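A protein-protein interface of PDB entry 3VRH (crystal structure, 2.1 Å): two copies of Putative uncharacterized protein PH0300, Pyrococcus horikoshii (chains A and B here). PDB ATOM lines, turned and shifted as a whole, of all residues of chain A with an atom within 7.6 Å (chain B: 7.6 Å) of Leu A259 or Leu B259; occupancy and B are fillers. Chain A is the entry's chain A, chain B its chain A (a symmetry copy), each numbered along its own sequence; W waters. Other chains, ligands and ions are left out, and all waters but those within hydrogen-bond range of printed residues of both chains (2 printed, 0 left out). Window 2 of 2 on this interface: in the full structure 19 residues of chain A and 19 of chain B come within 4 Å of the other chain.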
ATOM      1  N   TRP A 171     -24.757  -5.031   3.579  1.00  0.00           N
ATOM      2  CA  TRP A 171     -24.140  -4.903   4.898  1.00  0.00           C
ATOM      3  C   TRP A 171     -22.601  -4.779   4.858  1.00  0.00           C
ATOM      4  O   TRP A 171     -21.883  -5.480   5.568  1.00  0.00           O
ATOM      5  CB  TRP A 171     -24.650  -5.997   5.848  1.00  0.00           C
ATOM      6  CG  TRP A 171     -26.107  -5.756   6.146  1.00  0.00           C
ATOM      7  CD1 TRP A 171     -27.193  -6.343   5.544  1.00  0.00           C
ATOM      8  CD2 TRP A 171     -26.628  -4.783   7.054  1.00  0.00           C
ATOM      9  NE1 TRP A 171     -28.363  -5.804   6.046  1.00  0.00           N
ATOM     10  CE2 TRP A 171     -28.041  -4.853   6.982  1.00  0.00           C
ATOM     11  CE3 TRP A 171     -26.037  -3.857   7.924  1.00  0.00           C
ATOM     12  CZ2 TRP A 171     -28.863  -4.040   7.754  1.00  0.00           C
ATOM     13  CZ3 TRP A 171     -26.856  -3.043   8.682  1.00  0.00           C
ATOM     14  CH2 TRP A 171     -28.256  -3.144   8.597  1.00  0.00           C
ATOM     15  N   THR A 173     -20.318  -2.981   6.297  1.00  0.00           N
ATOM     16  CA  THR A 173     -20.237  -2.089   7.435  1.00  0.00           C
ATOM     17  C   THR A 173     -18.903  -1.358   7.475  1.00  0.00           C
ATOM     18  O   THR A 173     -18.813  -0.258   8.033  1.00  0.00           O
ATOM     19  CB  THR A 173     -20.477  -2.844   8.742  1.00  0.00           C
ATOM     20  OG1 THR A 173     -19.587  -3.961   8.806  1.00  0.00           O
ATOM     21  CG2 THR A 173     -21.915  -3.357   8.777  1.00  0.00           C
ATOM     22  N   GLU A 174     -17.876  -1.959   6.871  1.00  0.00           N
ATOM     23  CA  GLU A 174     -16.576  -1.297   6.781  1.00  0.00           C
ATOM     24  C   GLU A 174     -16.667  -0.044   5.929  1.00  0.00           C
ATOM     25  O   GLU A 174     -16.309   1.044   6.376  1.00  0.00           O
ATOM     26  CB  GLU A 174     -15.502  -2.249   6.251  1.00  0.00           C
ATOM     27  CG  GLU A 174     -14.867  -3.082   7.362  1.00  0.00           C
ATOM     28  CD  GLU A 174     -13.548  -3.720   6.960  1.00  0.00           C
ATOM     29  OE1 GLU A 174     -13.060  -3.438   5.837  1.00  0.00           O
ATOM     30  OE2 GLU A 174     -13.003  -4.504   7.775  1.00  0.00           O
ATOM     31  N   LEU A 176     -19.320   1.501   5.343  1.00  0.00           N
ATOM     32  CA  LEU A 176     -20.287   2.370   6.017  1.00  0.00           C
ATOM     33  C   LEU A 176     -19.651   3.240   7.096  1.00  0.00           C
ATOM     34  O   LEU A 176     -20.204   4.282   7.474  1.00  0.00           O
ATOM     35  CB  LEU A 176     -21.431   1.549   6.638  1.00  0.00           C
ATOM     36  CG  LEU A 176     -22.427   0.912   5.664  1.00  0.00           C
ATOM     37  CD1 LEU A 176     -23.376  -0.009   6.416  1.00  0.00           C
ATOM     38  CD2 LEU A 176     -23.185   1.979   4.899  1.00  0.00           C
ATOM     39  N   ALA A 177     -18.509   2.804   7.617  1.00  0.00           N
ATOM     40  CA  ALA A 177     -17.831   3.584   8.641  1.00  0.00           C
ATOM     41  C   ALA A 177     -17.139   4.785   8.007  1.00  0.00           C
ATOM     42  O   ALA A 177     -16.884   5.788   8.668  1.00  0.00           O
ATOM     43  CB  ALA A 177     -16.837   2.724   9.398  1.00  0.00           C
ATOM     44  N   TYR A 253     -27.872   9.211   8.452  1.00  0.00           N
ATOM     45  CA  TYR A 253     -26.634   8.439   8.372  1.00  0.00           C
ATOM     46  C   TYR A 253     -25.453   9.115   9.079  1.00  0.00           C
ATOM     47  O   TYR A 253     -24.653   8.447   9.756  1.00  0.00           O
ATOM     48  CB  TYR A 253     -26.245   8.166   6.915  1.00  0.00           C
ATOM     49  CG  TYR A 253     -24.814   7.690   6.792  1.00  0.00           C
ATOM     50  CD1 TYR A 253     -24.445   6.431   7.238  1.00  0.00           C
ATOM     51  CD2 TYR A 253     -23.834   8.510   6.251  1.00  0.00           C
ATOM     52  CE1 TYR A 253     -23.142   5.993   7.148  1.00  0.00           C
ATOM     53  CE2 TYR A 253     -22.539   8.082   6.140  1.00  0.00           C
ATOM     54  CZ  TYR A 253     -22.193   6.826   6.590  1.00  0.00           C
ATOM     55  OH  TYR A 253     -20.884   6.407   6.485  1.00  0.00           O
ATOM     56  N   LYS A 255     -25.475  11.098  11.502  1.00  0.00           N
ATOM     57  CA  LYS A 255     -25.694  11.043  12.944  1.00  0.00           C
ATOM     58  C   LYS A 255     -25.379   9.676  13.555  1.00  0.00           C
ATOM     59  O   LYS A 255     -25.041   9.579  14.734  1.00  0.00           O
ATOM     60  CB  LYS A 255     -27.128  11.481  13.266  1.00  0.00           C
ATOM     61  CG  LYS A 255     -27.460  12.879  12.711  1.00  0.00           C
ATOM     62  CD  LYS A 255     -28.855  13.388  13.087  1.00  0.00           C
ATOM     63  CE  LYS A 255     -28.837  14.124  14.423  1.00  0.00           C
ATOM     64  NZ  LYS A 255     -28.453  13.204  15.550  1.00  0.00           N
ATOM     65  N   LYS A 256     -25.464   8.625  12.745  1.00  0.00           N
ATOM     66  CA  LYS A 256     -25.351   7.258  13.261  1.00  0.00           C
ATOM     67  C   LYS A 256     -24.083   6.575  12.799  1.00  0.00           C
ATOM     68  O   LYS A 256     -23.810   5.449  13.208  1.00  0.00           O
ATOM     69  CB  LYS A 256     -26.548   6.409  12.819  1.00  0.00           C
ATOM     70  CG  LYS A 256     -27.903   6.911  13.278  1.00  0.00           C
ATOM     71  CD  LYS A 256     -27.903   7.180  14.775  1.00  0.00           C
ATOM     72  CE  LYS A 256     -29.313   7.359  15.301  1.00  0.00           C
ATOM     73  NZ  LYS A 256     -29.251   7.551  16.764  1.00  0.00           N
ATOM     74  N   LYS A 257     -23.345   7.256  11.922  1.00  0.00           N
ATOM     75  CA  LYS A 257     -22.132   6.745  11.285  1.00  0.00           C
ATOM     76  C   LYS A 257     -21.193   6.070  12.286  1.00  0.00           C
ATOM     77  O   LYS A 257     -20.548   5.055  11.993  1.00  0.00           O
ATOM     78  CB  LYS A 257     -21.408   7.918  10.602  1.00  0.00           C
ATOM     79  CG  LYS A 257     -20.213   7.546   9.766  1.00  0.00           C
ATOM     80  CD  LYS A 257     -19.846   8.690   8.800  1.00  0.00           C
ATOM     81  CE  LYS A 257     -18.908   9.712   9.442  1.00  0.00           C
ATOM     82  NZ  LYS A 257     -17.619   9.054   9.795  1.00  0.00           N
ATOM     83  N   LYS A 258     -21.139   6.651  13.476  1.00  0.00           N
ATOM     84  CA  LYS A 258     -20.285   6.194  14.561  1.00  0.00           C
ATOM     85  C   LYS A 258     -20.429   4.702  14.889  1.00  0.00           C
ATOM     86  O   LYS A 258     -19.476   4.059  15.330  1.00  0.00           O
ATOM     87  CB  LYS A 258     -20.601   7.033  15.799  1.00  0.00           C
ATOM     88  CG  LYS A 258     -21.221   8.405  15.464  1.00  0.00           C
ATOM     89  CD  LYS A 258     -20.840   9.462  16.508  1.00  0.00           C
ATOM     90  CE  LYS A 258     -19.319   9.675  16.563  1.00  0.00           C
ATOM     91  NZ  LYS A 258     -18.864  10.569  17.678  1.00  0.00           N
ATOM     92  N   LEU A 259     -21.628   4.160  14.665  1.00  0.00           N
ATOM     93  CA  LEU A 259     -21.953   2.780  15.043  1.00  0.00           C
ATOM     94  C   LEU A 259     -21.214   1.749  14.215  1.00  0.00           C
ATOM     95  O   LEU A 259     -21.152   0.580  14.587  1.00  0.00           O
ATOM     96  CB  LEU A 259     -23.468   2.527  14.941  1.00  0.00           C
ATOM     97  CG  LEU A 259     -24.379   3.309  15.900  1.00  0.00           C
ATOM     98  CD1 LEU A 259     -25.855   3.195  15.510  1.00  0.00           C
ATOM     99  CD2 LEU A 259     -24.164   2.860  17.345  1.00  0.00           C
ATOM    100  N   PHE A 260     -20.666   2.176  13.084  1.00  0.00           N
ATOM    101  CA  PHE A 260     -19.960   1.250  12.214  1.00  0.00           C
ATOM    102  C   PHE A 260     -18.463   1.296  12.468  1.00  0.00           C
ATOM    103  O   PHE A 260     -17.708   0.516  11.898  1.00  0.00           O
ATOM    104  CB  PHE A 260     -20.290   1.537  10.745  1.00  0.00           C
ATOM    105  CG  PHE A 260     -21.756   1.472  10.446  1.00  0.00           C
ATOM    106  CD1 PHE A 260     -22.498   2.633  10.274  1.00  0.00           C
ATOM    107  CD2 PHE A 260     -22.406   0.248  10.383  1.00  0.00           C
ATOM    108  CE1 PHE A 260     -23.866   2.568  10.021  1.00  0.00           C
ATOM    109  CE2 PHE A 260     -23.767   0.175  10.144  1.00  0.00           C
ATOM    110  CZ  PHE A 260     -24.501   1.330   9.958  1.00  0.00           C
ATOM    111  N   GLU A 261     -18.050   2.203  13.346  1.00  0.00           N
ATOM    112  CA  GLU A 261     -16.622   2.469  13.571  1.00  0.00           C
ATOM    113  C   GLU A 261     -15.758   1.332  14.159  1.00  0.00           C
ATOM    114  O   GLU A 261     -14.549   1.298  13.906  1.00  0.00           O
ATOM    115  CB  GLU A 261     -16.413   3.800  14.316  1.00  0.00           C
ATOM    116  CG  GLU A 261     -16.887   5.003  13.490  1.00  0.00           C
ATOM    117  CD  GLU A 261     -16.514   6.360  14.081  1.00  0.00           C
ATOM    118  OE1 GLU A 261     -15.878   6.391  15.162  1.00  0.00           O
ATOM    119  OE2 GLU A 261     -16.860   7.395  13.454  1.00  0.00           O
ATOM    120  N   PRO A 262     -16.356   0.409  14.944  1.00  0.00           N
ATOM    121  CA  PRO A 262     -15.574  -0.794  15.253  1.00  0.00           C
ATOM    122  C   PRO A 262     -15.805  -1.910  14.229  1.00  0.00           C
ATOM    123  O   PRO A 262     -15.713  -1.670  13.021  1.00  0.00           O
ATOM    124  CB  PRO A 262     -16.118  -1.213  16.618  1.00  0.00           C
ATOM    125  CG  PRO A 262     -17.541  -0.787  16.576  1.00  0.00           C
ATOM    126  CD  PRO A 262     -17.546   0.518  15.811  1.00  0.00           C
ATOM    127  N   TRP B 171     -33.140   5.804   9.869  1.00  0.00           N
ATOM    128  CA  TRP B 171     -32.156   5.540  10.917  1.00  0.00           C
ATOM    129  C   TRP B 171     -32.774   5.338  12.318  1.00  0.00           C
ATOM    130  O   TRP B 171     -32.348   5.942  13.300  1.00  0.00           O
ATOM    131  CB  TRP B 171     -31.027   6.581  10.881  1.00  0.00           C
ATOM    132  CG  TRP B 171     -30.220   6.395   9.623  1.00  0.00           C
ATOM    133  CD1 TRP B 171     -30.340   7.085   8.441  1.00  0.00           C
ATOM    134  CD2 TRP B 171     -29.236   5.383   9.399  1.00  0.00           C
ATOM    135  NE1 TRP B 171     -29.467   6.571   7.501  1.00  0.00           N
ATOM    136  CE2 TRP B 171     -28.771   5.534   8.070  1.00  0.00           C
ATOM    137  CE3 TRP B 171     -28.700   4.362  10.195  1.00  0.00           C
ATOM    138  CZ2 TRP B 171     -27.791   4.707   7.530  1.00  0.00           C
ATOM    139  CZ3 TRP B 171     -27.735   3.536   9.653  1.00  0.00           C
ATOM    140  CH2 TRP B 171     -27.285   3.717   8.333  1.00  0.00           C
ATOM    141  N   THR B 173     -32.390   3.314  14.822  1.00  0.00           N
ATOM    142  CA  THR B 173     -31.414   2.333  15.247  1.00  0.00           C
ATOM    143  C   THR B 173     -31.915   1.532  16.440  1.00  0.00           C
ATOM    144  O   THR B 173     -31.490   0.388  16.644  1.00  0.00           O
ATOM    145  CB  THR B 173     -30.074   2.995  15.566  1.00  0.00           C
ATOM    146  OG1 THR B 173     -30.288   4.054  16.502  1.00  0.00           O
ATOM    147  CG2 THR B 173     -29.477   3.579  14.288  1.00  0.00           C
ATOM    148  N   GLU B 174     -32.825   2.122  17.216  1.00  0.00           N
ATOM    149  CA  GLU B 174     -33.430   1.401  18.334  1.00  0.00           C
ATOM    150  C   GLU B 174     -34.251   0.225  17.837  1.00  0.00           C
ATOM    151  O   GLU B 174     -34.028  -0.911  18.248  1.00  0.00           O
ATOM    152  CB  GLU B 174     -34.272   2.334  19.207  1.00  0.00           C
ATOM    153  CG  GLU B 174     -33.436   3.042  20.271  1.00  0.00           C
ATOM    154  CD  GLU B 174     -34.267   3.639  21.393  1.00  0.00           C
ATOM    155  OE1 GLU B 174     -35.504   3.421  21.409  1.00  0.00           O
ATOM    156  OE2 GLU B 174     -33.674   4.327  22.261  1.00  0.00           O
ATOM    157  N   LEU B 176     -33.884  -1.126  15.042  1.00  0.00           N
ATOM    158  CA  LEU B 176     -32.945  -1.992  14.328  1.00  0.00           C
ATOM    159  C   LEU B 176     -32.230  -2.976  15.247  1.00  0.00           C
ATOM    160  O   LEU B 176     -31.728  -4.015  14.793  1.00  0.00           O
ATOM    161  CB  LEU B 176     -31.899  -1.163  13.562  1.00  0.00           C
ATOM    162  CG  LEU B 176     -32.394  -0.400  12.330  1.00  0.00           C
ATOM    163  CD1 LEU B 176     -31.295   0.509  11.802  1.00  0.00           C
ATOM    164  CD2 LEU B 176     -32.876  -1.362  11.262  1.00  0.00           C
ATOM    165  N   ALA B 177     -32.151  -2.644  16.531  1.00  0.00           N
ATOM    166  CA  ALA B 177     -31.498  -3.537  17.475  1.00  0.00           C
ATOM    167  C   ALA B 177     -32.407  -4.719  17.789  1.00  0.00           C
ATOM    168  O   ALA B 177     -31.943  -5.784  18.190  1.00  0.00           O
ATOM    169  CB  ALA B 177     -31.122  -2.793  18.744  1.00  0.00           C
ATOM    170  N   TYR B 253     -28.218  -8.592   7.667  1.00  0.00           N
ATOM    171  CA  TYR B 253     -28.713  -7.882   8.845  1.00  0.00           C
ATOM    172  C   TYR B 253     -28.536  -8.673  10.146  1.00  0.00           C
ATOM    173  O   TYR B 253     -28.173  -8.104  11.189  1.00  0.00           O
ATOM    174  CB  TYR B 253     -30.194  -7.516   8.688  1.00  0.00           C
ATOM    175  CG  TYR B 253     -30.817  -7.109  10.005  1.00  0.00           C
ATOM    176  CD1 TYR B 253     -30.475  -5.910  10.610  1.00  0.00           C
ATOM    177  CD2 TYR B 253     -31.728  -7.935  10.649  1.00  0.00           C
ATOM    178  CE1 TYR B 253     -31.022  -5.537  11.818  1.00  0.00           C
ATOM    179  CE2 TYR B 253     -32.292  -7.569  11.840  1.00  0.00           C
ATOM    180  CZ  TYR B 253     -31.938  -6.372  12.425  1.00  0.00           C
ATOM    181  OH  TYR B 253     -32.502  -6.016  13.631  1.00  0.00           O
ATOM    182  N   LYS B 255     -26.389 -10.836  10.865  1.00  0.00           N
ATOM    183  CA  LYS B 255     -24.969 -10.883  11.198  1.00  0.00           C
ATOM    184  C   LYS B 255     -24.448  -9.587  11.823  1.00  0.00           C
ATOM    185  O   LYS B 255     -23.478  -9.600  12.579  1.00  0.00           O
ATOM    186  CB  LYS B 255     -24.158 -11.268   9.955  1.00  0.00           C
ATOM    187  CG  LYS B 255     -24.622 -12.599   9.334  1.00  0.00           C
ATOM    188  CD  LYS B 255     -23.780 -13.060   8.140  1.00  0.00           C
ATOM    189  CE  LYS B 255     -22.588 -13.899   8.593  1.00  0.00           C
ATOM    190  NZ  LYS B 255     -21.640 -13.092   9.436  1.00  0.00           N
ATOM    191  N   LYS B 256     -25.111  -8.472  11.528  1.00  0.00           N
ATOM    192  CA  LYS B 256     -24.603  -7.157  11.930  1.00  0.00           C
ATOM    193  C   LYS B 256     -25.469  -6.509  12.987  1.00  0.00           C
ATOM    194  O   LYS B 256     -25.132  -5.434  13.479  1.00  0.00           O
ATOM    195  CB  LYS B 256     -24.520  -6.215  10.725  1.00  0.00           C
ATOM    196  CG  LYS B 256     -23.616  -6.679   9.600  1.00  0.00           C
ATOM    197  CD  LYS B 256     -22.243  -7.063  10.132  1.00  0.00           C
ATOM    198  CE  LYS B 256     -21.239  -7.209   9.006  1.00  0.00           C
ATOM    199  NZ  LYS B 256     -19.917  -7.517   9.589  1.00  0.00           N
ATOM    200  N   LYS B 257     -26.593  -7.157  13.293  1.00  0.00           N
ATOM    201  CA  LYS B 257     -27.609  -6.663  14.221  1.00  0.00           C
ATOM    202  C   LYS B 257     -26.997  -6.120  15.514  1.00  0.00           C
ATOM    203  O   LYS B 257     -27.456  -5.120  16.082  1.00  0.00           O
ATOM    204  CB  LYS B 257     -28.575  -7.815  14.548  1.00  0.00           C
ATOM    205  CG  LYS B 257     -29.775  -7.443  15.375  1.00  0.00           C
ATOM    206  CD  LYS B 257     -30.867  -8.526  15.268  1.00  0.00           C
ATOM    207  CE  LYS B 257     -30.678  -9.643  16.294  1.00  0.00           C
ATOM    208  NZ  LYS B 257     -30.798  -9.084  17.669  1.00  0.00           N
ATOM    209  N   LYS B 258     -25.946  -6.793  15.957  1.00  0.00           N
ATOM    210  CA  LYS B 258     -25.237  -6.469  17.185  1.00  0.00           C
ATOM    211  C   LYS B 258     -24.800  -5.002  17.289  1.00  0.00           C
ATOM    212  O   LYS B 258     -24.713  -4.447  18.386  1.00  0.00           O
ATOM    213  CB  LYS B 258     -24.016  -7.384  17.283  1.00  0.00           C
ATOM    214  CG  LYS B 258     -24.167  -8.691  16.478  1.00  0.00           C
ATOM    215  CD  LYS B 258     -23.399  -9.845  17.133  1.00  0.00           C
ATOM    216  CE  LYS B 258     -23.928 -10.142  18.545  1.00  0.00           C
ATOM    217  NZ  LYS B 258     -23.113 -11.144  19.308  1.00  0.00           N
ATOM    218  N   LEU B 259     -24.530  -4.381  16.139  1.00  0.00           N
ATOM    219  CA  LEU B 259     -23.986  -3.020  16.085  1.00  0.00           C
ATOM    220  C   LEU B 259     -24.974  -1.968  16.545  1.00  0.00           C
ATOM    221  O   LEU B 259     -24.590  -0.837  16.832  1.00  0.00           O
ATOM    222  CB  LEU B 259     -23.501  -2.680  14.665  1.00  0.00           C
ATOM    223  CG  LEU B 259     -22.313  -3.485  14.114  1.00  0.00           C
ATOM    224  CD1 LEU B 259     -22.117  -3.262  12.613  1.00  0.00           C
ATOM    225  CD2 LEU B 259     -21.032  -3.163  14.882  1.00  0.00           C
ATOM    226  N   PHE B 260     -26.249  -2.333  16.602  1.00  0.00           N
ATOM    227  CA  PHE B 260     -27.269  -1.380  17.007  1.00  0.00           C
ATOM    228  C   PHE B 260     -27.596  -1.526  18.483  1.00  0.00           C
ATOM    229  O   PHE B 260     -28.365  -0.744  19.033  1.00  0.00           O
ATOM    230  CB  PHE B 260     -28.522  -1.534  16.136  1.00  0.00           C
ATOM    231  CG  PHE B 260     -28.247  -1.368  14.673  1.00  0.00           C
ATOM    232  CD1 PHE B 260     -28.191  -2.471  13.832  1.00  0.00           C
ATOM    233  CD2 PHE B 260     -27.997  -0.110  14.144  1.00  0.00           C
ATOM    234  CE1 PHE B 260     -27.909  -2.313  12.476  1.00  0.00           C
ATOM    235  CE2 PHE B 260     -27.706   0.054  12.802  1.00  0.00           C
ATOM    236  CZ  PHE B 260     -27.665  -1.043  11.962  1.00  0.00           C
ATOM    237  N   GLU B 261     -26.985  -2.519  19.119  1.00  0.00           N
ATOM    238  CA  GLU B 261     -27.325  -2.878  20.503  1.00  0.00           C
ATOM    239  C   GLU B 261     -27.043  -1.837  21.610  1.00  0.00           C
ATOM    240  O   GLU B 261     -27.727  -1.848  22.638  1.00  0.00           O
ATOM    241  CB  GLU B 261     -26.783  -4.272  20.867  1.00  0.00           C
ATOM    242  CG  GLU B 261     -27.435  -5.380  20.029  1.00  0.00           C
ATOM    243  CD  GLU B 261     -27.099  -6.797  20.487  1.00  0.00           C
ATOM    244  OE1 GLU B 261     -26.337  -6.946  21.472  1.00  0.00           O
ATOM    245  OE2 GLU B 261     -27.605  -7.759  19.853  1.00  0.00           O
ATOM    246  N   PRO B 262     -26.044  -0.949  21.418  1.00  0.00           N
ATOM    247  CA  PRO B 262     -25.986   0.184  22.351  1.00  0.00           C
ATOM    248  C   PRO B 262     -26.788   1.388  21.846  1.00  0.00           C
ATOM    249  O   PRO B 262     -27.955   1.238  21.467  1.00  0.00           O
ATOM    250  CB  PRO B 262     -24.496   0.522  22.383  1.00  0.00           C
ATOM    251  CG  PRO B 262     -24.026   0.177  21.017  1.00  0.00           C
ATOM    252  CD  PRO B 262     -24.802  -1.062  20.628  1.00  0.00           C
HETATM  253  O   HOH W   1     -27.739   4.845  18.234  1.00  0.00           O
HETATM  254  O   HOH W   2     -18.977  -5.019  11.744  1.00  0.00           O
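N of Tyr A253 lies close to NE1 of Trp B171.
The indole nitrogen (NE1) of Trp A171 lies close to the backbone NH (N) of Tyr B253 (3.2 Å).
O of Leu B176 is in hydrogen-bond range of OH of Tyr B253, at 2.4 Å.
O of Leu A176 is in hydrogen-bond range of OH of Tyr A253.
Lys B256 touches Trp A171.
Trp A171 touches Phe B260 (CZ3 to CZ, 3.9 Å).
Thr A173 touches Lys B256 (OG1 to CE, 3.6 Å).
Thr A173 touches Leu B259.
Lys A256 touches Trp B171 (CE to O, 3.9 Å).
Lys A256 touches Thr B173 (CE to OG1, 3.6 Å).
Leu A259 touches Thr B173 (CD1 to CG2, 3.8 Å).
Leu B259 touches Leu A259.
CZ3 of Trp B171 touches CZ of Phe A260, 3.9 Å away.
Leu A259 touches just these residues of chain B: Thr B173 and Leu B259.
Of chain A, only Thr A173 and Leu A259 come within 4 Å of Leu B259.
Of the printed residues of chain B, Phe A260 touches Trp B171.
Of the printed residues of chain A, Phe B260 touches Trp A171 (3.9 Å).
Of the printed residues of chain A, Tyr B253 touches Trp A171 (3.2 Å).
Of the printed residues of chain B, Lys A256 touches Trp B171 (3.9 Å) and Thr B173 (3.6 Å).
Of the printed residues of chain A, Trp B171 touches Tyr A253, Lys A256 and Phe A260.
Glu A261 touches none of the printed residues of chain B.
The nearest residue of chain A that does not touch Leu B259 is Phe A260 (4.2 Å).
The nearest printed residue of chain B that does not touch Thr A173 is Phe B260 (7.0 Å).
Of the 14 printed residues of chain B, 6 touch a printed residue of chain A.
Printed residues of chain A that touch a printed residue of chain B: Trp A171, Thr A173, Tyr A253, Lys A256, Leu A259 and Phe A260.
Hydrophobic or aromatic side chains of chain A that line the printed part of chain B: Trp A171, Tyr A253, Leu A259 and Phe A260.
Among the printed residues, 11 pairs touch across the chains.
Trp A171 touches Lys B256, and with the chains exchanged Lys A256 touches Trp B171.
Trp A171 touches Phe B260, and with the chains exchanged Phe A260 touches Trp B171.
Thr A173 touches Leu B259, and with the chains exchanged Leu A259 touches Thr B173.
Leu B259 touches its own counterpart, Leu A259.
14 positions are printed for both chains.
Of the 11 pairs that touch across the chains among the printed residues, 11 have their exchanged pair printed and touching as well.
Water W2 lies within hydrogen-bond range of the side-chain hydroxyl (OG1) of Thr A173 and the side-chain amino group (NZ) of Lys B256.
Water W1 bridges OG1 of Thr B173 (3.2 Å) and NZ of Lys A256 (3.4 Å).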
